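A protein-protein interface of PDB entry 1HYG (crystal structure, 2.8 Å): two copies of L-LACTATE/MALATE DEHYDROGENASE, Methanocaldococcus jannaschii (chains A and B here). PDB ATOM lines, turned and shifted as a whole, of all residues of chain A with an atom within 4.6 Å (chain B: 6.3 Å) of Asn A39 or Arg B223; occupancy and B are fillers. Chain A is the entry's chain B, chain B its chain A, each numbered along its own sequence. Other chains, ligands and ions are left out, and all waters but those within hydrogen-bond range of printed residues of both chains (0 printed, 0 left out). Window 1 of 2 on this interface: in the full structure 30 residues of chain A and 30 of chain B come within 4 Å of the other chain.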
ATOM      1  N   SER A  37      -7.672 -23.734  26.729  1.00  0.00           N
ATOM      2  CA  SER A  37      -8.134 -22.386  26.454  1.00  0.00           C
ATOM      3  C   SER A  37      -7.639 -21.934  25.080  1.00  0.00           C
ATOM      4  O   SER A  37      -7.351 -20.759  24.864  1.00  0.00           O
ATOM      5  CB  SER A  37      -7.635 -21.432  27.531  1.00  0.00           C
ATOM      6  OG  SER A  37      -6.228 -21.353  27.472  1.00  0.00           O
ATOM      7  N   ILE A  38      -7.543 -22.877  24.151  1.00  0.00           N
ATOM      8  CA  ILE A  38      -7.098 -22.558  22.809  1.00  0.00           C
ATOM      9  C   ILE A  38      -8.261 -22.054  21.970  1.00  0.00           C
ATOM     10  O   ILE A  38      -8.072 -21.286  21.028  1.00  0.00           O
ATOM     11  CB  ILE A  38      -6.470 -23.779  22.135  1.00  0.00           C
ATOM     12  CG1 ILE A  38      -5.141 -24.108  22.818  1.00  0.00           C
ATOM     13  CG2 ILE A  38      -6.271 -23.522  20.658  1.00  0.00           C
ATOM     14  CD1 ILE A  38      -4.114 -22.982  22.768  1.00  0.00           C
ATOM     15  N   ASN A  39      -9.470 -22.478  22.307  1.00  0.00           N
ATOM     16  CA  ASN A  39     -10.631 -22.026  21.559  1.00  0.00           C
ATOM     17  C   ASN A  39     -10.964 -20.597  21.932  1.00  0.00           C
ATOM     18  O   ASN A  39     -11.512 -19.844  21.127  1.00  0.00           O
ATOM     19  CB  ASN A  39     -11.831 -22.935  21.823  1.00  0.00           C
ATOM     20  CG  ASN A  39     -11.796 -24.191  20.967  1.00  0.00           C
ATOM     21  OD1 ASN A  39     -10.918 -24.338  20.097  1.00  0.00           O
ATOM     22  ND2 ASN A  39     -12.753 -25.100  21.195  1.00  0.00           N
ATOM     23  N   LYS A  40     -10.621 -20.223  23.159  1.00  0.00           N
ATOM     24  CA  LYS A  40     -10.886 -18.871  23.612  1.00  0.00           C
ATOM     25  C   LYS A  40      -9.948 -17.901  22.875  1.00  0.00           C
ATOM     26  O   LYS A  40     -10.302 -16.749  22.628  1.00  0.00           O
ATOM     27  CB  LYS A  40     -10.707 -18.785  25.138  1.00  0.00           C
ATOM     28  CG  LYS A  40     -10.941 -17.391  25.707  1.00  0.00           C
ATOM     29  CD  LYS A  40     -12.042 -17.350  26.761  1.00  0.00           C
ATOM     30  CE  LYS A  40     -11.642 -18.036  28.067  1.00  0.00           C
ATOM     31  NZ  LYS A  40     -11.581 -19.520  27.942  1.00  0.00           N
ATOM     32  N   LEU A  41      -8.765 -18.381  22.506  1.00  0.00           N
ATOM     33  CA  LEU A  41      -7.804 -17.549  21.800  1.00  0.00           C
ATOM     34  C   LEU A  41      -8.201 -17.397  20.343  1.00  0.00           C
ATOM     35  O   LEU A  41      -8.193 -16.293  19.801  1.00  0.00           O
ATOM     36  CB  LEU A  41      -6.393 -18.148  21.867  1.00  0.00           C
ATOM     37  CG  LEU A  41      -5.729 -18.383  23.226  1.00  0.00           C
ATOM     38  CD1 LEU A  41      -4.271 -18.725  22.983  1.00  0.00           C
ATOM     39  CD2 LEU A  41      -5.826 -17.149  24.114  1.00  0.00           C
ATOM     40  N   GLU A  42      -8.535 -18.506  19.698  1.00  0.00           N
ATOM     41  CA  GLU A  42      -8.926 -18.432  18.306  1.00  0.00           C
ATOM     42  C   GLU A  42     -10.177 -17.573  18.267  1.00  0.00           C
ATOM     43  O   GLU A  42     -10.442 -16.873  17.283  1.00  0.00           O
ATOM     44  CB  GLU A  42      -9.192 -19.831  17.744  1.00  0.00           C
ATOM     45  CG  GLU A  42      -7.990 -20.780  17.881  1.00  0.00           C
ATOM     46  CD  GLU A  42      -7.958 -21.895  16.838  1.00  0.00           C
ATOM     47  OE1 GLU A  42      -7.844 -21.574  15.630  1.00  0.00           O
ATOM     48  OE2 GLU A  42      -8.037 -23.083  17.223  1.00  0.00           O
ATOM     49  N   GLY A  43     -10.933 -17.610  19.360  1.00  0.00           N
ATOM     50  CA  GLY A  43     -12.143 -16.814  19.442  1.00  0.00           C
ATOM     51  C   GLY A  43     -11.753 -15.355  19.561  1.00  0.00           C
ATOM     52  O   GLY A  43     -12.456 -14.456  19.083  1.00  0.00           O
ATOM     53  N   GLU A  46     -10.351 -14.026  16.061  1.00  0.00           N
ATOM     54  CA  GLU A  46     -11.425 -13.634  15.159  1.00  0.00           C
ATOM     55  C   GLU A  46     -12.033 -12.307  15.613  1.00  0.00           C
ATOM     56  O   GLU A  46     -12.347 -11.441  14.788  1.00  0.00           O
ATOM     57  CB  GLU A  46     -12.517 -14.712  15.113  1.00  0.00           C
ATOM     58  CG  GLU A  46     -12.136 -16.000  14.392  1.00  0.00           C
ATOM     59  CD  GLU A  46     -11.705 -15.762  12.955  1.00  0.00           C
ATOM     60  OE1 GLU A  46     -12.191 -14.778  12.344  1.00  0.00           O
ATOM     61  OE2 GLU A  46     -10.894 -16.566  12.435  1.00  0.00           O
ATOM     62  N   GLY B 218     -20.850 -15.829  14.135  1.00  0.00           N
ATOM     63  CA  GLY B 218     -21.444 -15.982  15.448  1.00  0.00           C
ATOM     64  C   GLY B 218     -20.620 -17.087  16.079  1.00  0.00           C
ATOM     65  O   GLY B 218     -21.032 -17.759  17.023  1.00  0.00           O
ATOM     66  N   GLU B 219     -19.437 -17.284  15.504  1.00  0.00           N
ATOM     67  CA  GLU B 219     -18.505 -18.284  15.974  1.00  0.00           C
ATOM     68  C   GLU B 219     -17.659 -17.719  17.113  1.00  0.00           C
ATOM     69  O   GLU B 219     -16.866 -18.436  17.715  1.00  0.00           O
ATOM     70  CB  GLU B 219     -17.626 -18.782  14.819  1.00  0.00           C
ATOM     71  CG  GLU B 219     -17.392 -17.770  13.717  1.00  0.00           C
ATOM     72  CD  GLU B 219     -16.654 -18.365  12.523  1.00  0.00           C
ATOM     73  OE1 GLU B 219     -15.547 -18.919  12.727  1.00  0.00           O
ATOM     74  OE2 GLU B 219     -17.177 -18.272  11.384  1.00  0.00           O
ATOM     75  N   GLN B 220     -17.826 -16.433  17.411  1.00  0.00           N
ATOM     76  CA  GLN B 220     -17.095 -15.843  18.528  1.00  0.00           C
ATOM     77  C   GLN B 220     -17.743 -16.492  19.731  1.00  0.00           C
ATOM     78  O   GLN B 220     -17.081 -16.894  20.686  1.00  0.00           O
ATOM     79  CB  GLN B 220     -17.316 -14.336  18.616  1.00  0.00           C
ATOM     80  CG  GLN B 220     -16.164 -13.489  18.142  1.00  0.00           C
ATOM     81  CD  GLN B 220     -15.980 -13.548  16.645  1.00  0.00           C
ATOM     82  OE1 GLN B 220     -15.157 -12.829  16.081  1.00  0.00           O
ATOM     83  NE2 GLN B 220     -16.750 -14.409  15.987  1.00  0.00           N
ATOM     84  N   ILE B 221     -19.064 -16.590  19.658  1.00  0.00           N
ATOM     85  CA  ILE B 221     -19.854 -17.191  20.719  1.00  0.00           C
ATOM     86  C   ILE B 221     -19.346 -18.604  20.979  1.00  0.00           C
ATOM     87  O   ILE B 221     -18.795 -18.886  22.041  1.00  0.00           O
ATOM     88  CB  ILE B 221     -21.349 -17.252  20.333  1.00  0.00           C
ATOM     89  CG1 ILE B 221     -21.879 -15.839  20.048  1.00  0.00           C
ATOM     90  CG2 ILE B 221     -22.138 -17.918  21.441  1.00  0.00           C
ATOM     91  CD1 ILE B 221     -21.312 -15.200  18.776  1.00  0.00           C
ATOM     92  N   ILE B 222     -19.519 -19.480  19.995  1.00  0.00           N
ATOM     93  CA  ILE B 222     -19.074 -20.855  20.143  1.00  0.00           C
ATOM     94  C   ILE B 222     -17.573 -20.966  20.428  1.00  0.00           C
ATOM     95  O   ILE B 222     -17.187 -21.665  21.360  1.00  0.00           O
ATOM     96  CB  ILE B 222     -19.470 -21.726  18.895  1.00  0.00           C
ATOM     97  CG1 ILE B 222     -18.434 -22.841  18.668  1.00  0.00           C
ATOM     98  CG2 ILE B 222     -19.675 -20.837  17.672  1.00  0.00           C
ATOM     99  CD1 ILE B 222     -18.668 -23.652  17.421  1.00  0.00           C
ATOM    100  N   ARG B 223     -16.730 -20.281  19.652  1.00  0.00           N
ATOM    101  CA  ARG B 223     -15.284 -20.361  19.879  1.00  0.00           C
ATOM    102  C   ARG B 223     -14.944 -19.753  21.230  1.00  0.00           C
ATOM    103  O   ARG B 223     -14.722 -18.550  21.353  1.00  0.00           O
ATOM    104  CB  ARG B 223     -14.506 -19.654  18.766  1.00  0.00           C
ATOM    105  CG  ARG B 223     -13.674 -20.599  17.900  1.00  0.00           C
ATOM    106  CD  ARG B 223     -12.988 -19.861  16.743  1.00  0.00           C
ATOM    107  NE  ARG B 223     -12.242 -20.765  15.858  1.00  0.00           N
ATOM    108  CZ  ARG B 223     -11.470 -20.380  14.837  1.00  0.00           C
ATOM    109  NH1 ARG B 223     -11.324 -19.091  14.543  1.00  0.00           N
ATOM    110  NH2 ARG B 223     -10.832 -21.291  14.107  1.00  0.00           N
ATOM    111  N   LEU B 224     -14.908 -20.624  22.232  1.00  0.00           N
ATOM    112  CA  LEU B 224     -14.631 -20.275  23.622  1.00  0.00           C
ATOM    113  C   LEU B 224     -14.589 -18.775  23.929  1.00  0.00           C
ATOM    114  O   LEU B 224     -13.598 -18.254  24.445  1.00  0.00           O
ATOM    115  CB  LEU B 224     -13.335 -20.954  24.096  1.00  0.00           C
ATOM    116  CG  LEU B 224     -13.397 -21.746  25.413  1.00  0.00           C
ATOM    117  CD1 LEU B 224     -11.985 -22.220  25.788  1.00  0.00           C
ATOM    118  CD2 LEU B 224     -13.995 -20.876  26.523  1.00  0.00           C
ATOM    119  N   LYS B 225     -15.678 -18.089  23.606  1.00  0.00           N
ATOM    120  CA  LYS B 225     -15.796 -16.668  23.877  1.00  0.00           C
ATOM    121  C   LYS B 225     -17.250 -16.381  24.195  1.00  0.00           C
ATOM    122  O   LYS B 225     -18.142 -17.085  23.731  1.00  0.00           O
ATOM    123  CB  LYS B 225     -15.365 -15.838  22.667  1.00  0.00           C
ATOM    124  CG  LYS B 225     -13.944 -15.304  22.723  1.00  0.00           C
ATOM    125  CD  LYS B 225     -13.769 -14.159  21.733  1.00  0.00           C
ATOM    126  CE  LYS B 225     -14.569 -12.915  22.141  1.00  0.00           C
ATOM    127  NZ  LYS B 225     -13.927 -12.159  23.252  1.00  0.00           N
ATOM    128  N   GLY B 226     -17.486 -15.349  24.990  1.00  0.00           N
ATOM    129  CA  GLY B 226     -18.848 -15.006  25.335  1.00  0.00           C
ATOM    130  C   GLY B 226     -19.695 -14.801  24.098  1.00  0.00           C
ATOM    131  O   GLY B 226     -20.817 -15.307  24.013  1.00  0.00           O
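NH1 of Arg B223 lies within salt-bridge range of OE2 of Glu A46.
The guanidinium group (NH2) of Arg B223 lies within salt-bridge range of the side-chain carboxylate (OE1) of Glu A42.
The side-chain amide oxygen of Gln B220 lies close to the backbone carbonyl oxygen of Glu A46.
O of Asn A39 lies close to O of Arg B223, 3.5 Å away.
The backbone carbonyl oxygen (O) of Gln B220 sits close to the backbone NH (N) of Lys B225.
Ser A37 touches Leu B224 (CA to CD1, 3.9 Å).
CB of Leu B224 touches C of Asn A39 (3.2 Å).
Leu B224 touches Lys A40.
Lys A40 touches Lys B225.
O of Gly A43 touches CG of Gln B220, 3.9 Å away.
Arg B223 touches Gly A43.
Lys B225 touches Gly A43 (CD to O, 3.0 Å).
Of chain B, only Arg B223 (3.4 Å) and Leu B224 (3.2 Å) come within 4 Å of Asn A39.
Of the printed residues of chain A, Arg B223 touches Asn A39, Glu A42, Gly A43 and Glu A46.
Of the printed residues of chain B, Lys A40 touches Leu B224 and Lys B225.
Of the printed residues of chain B, Glu A42 touches Arg B223.
Of the printed residues of chain B, Gly A43 touches Gln B220, Arg B223 and Lys B225.
Of the printed residues of chain A, Lys B225 touches Lys A40 (3.9 Å) and Gly A43 (3.0 Å).
Ile B222 touches none of the printed residues of chain A.
The nearest residue of chain B that does not touch Asn A39 is Lys B225 (5.2 Å).
Hydrophobic or aromatic side chains of chain B that line the printed part of chain A: Leu B224.
Among the printed residues, 11 pairs touch across the chains.
No position is printed for both chains.
Of the 11 pairs that touch across the chains among the printed residues, none has its exchanged pair printed and touching as well.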
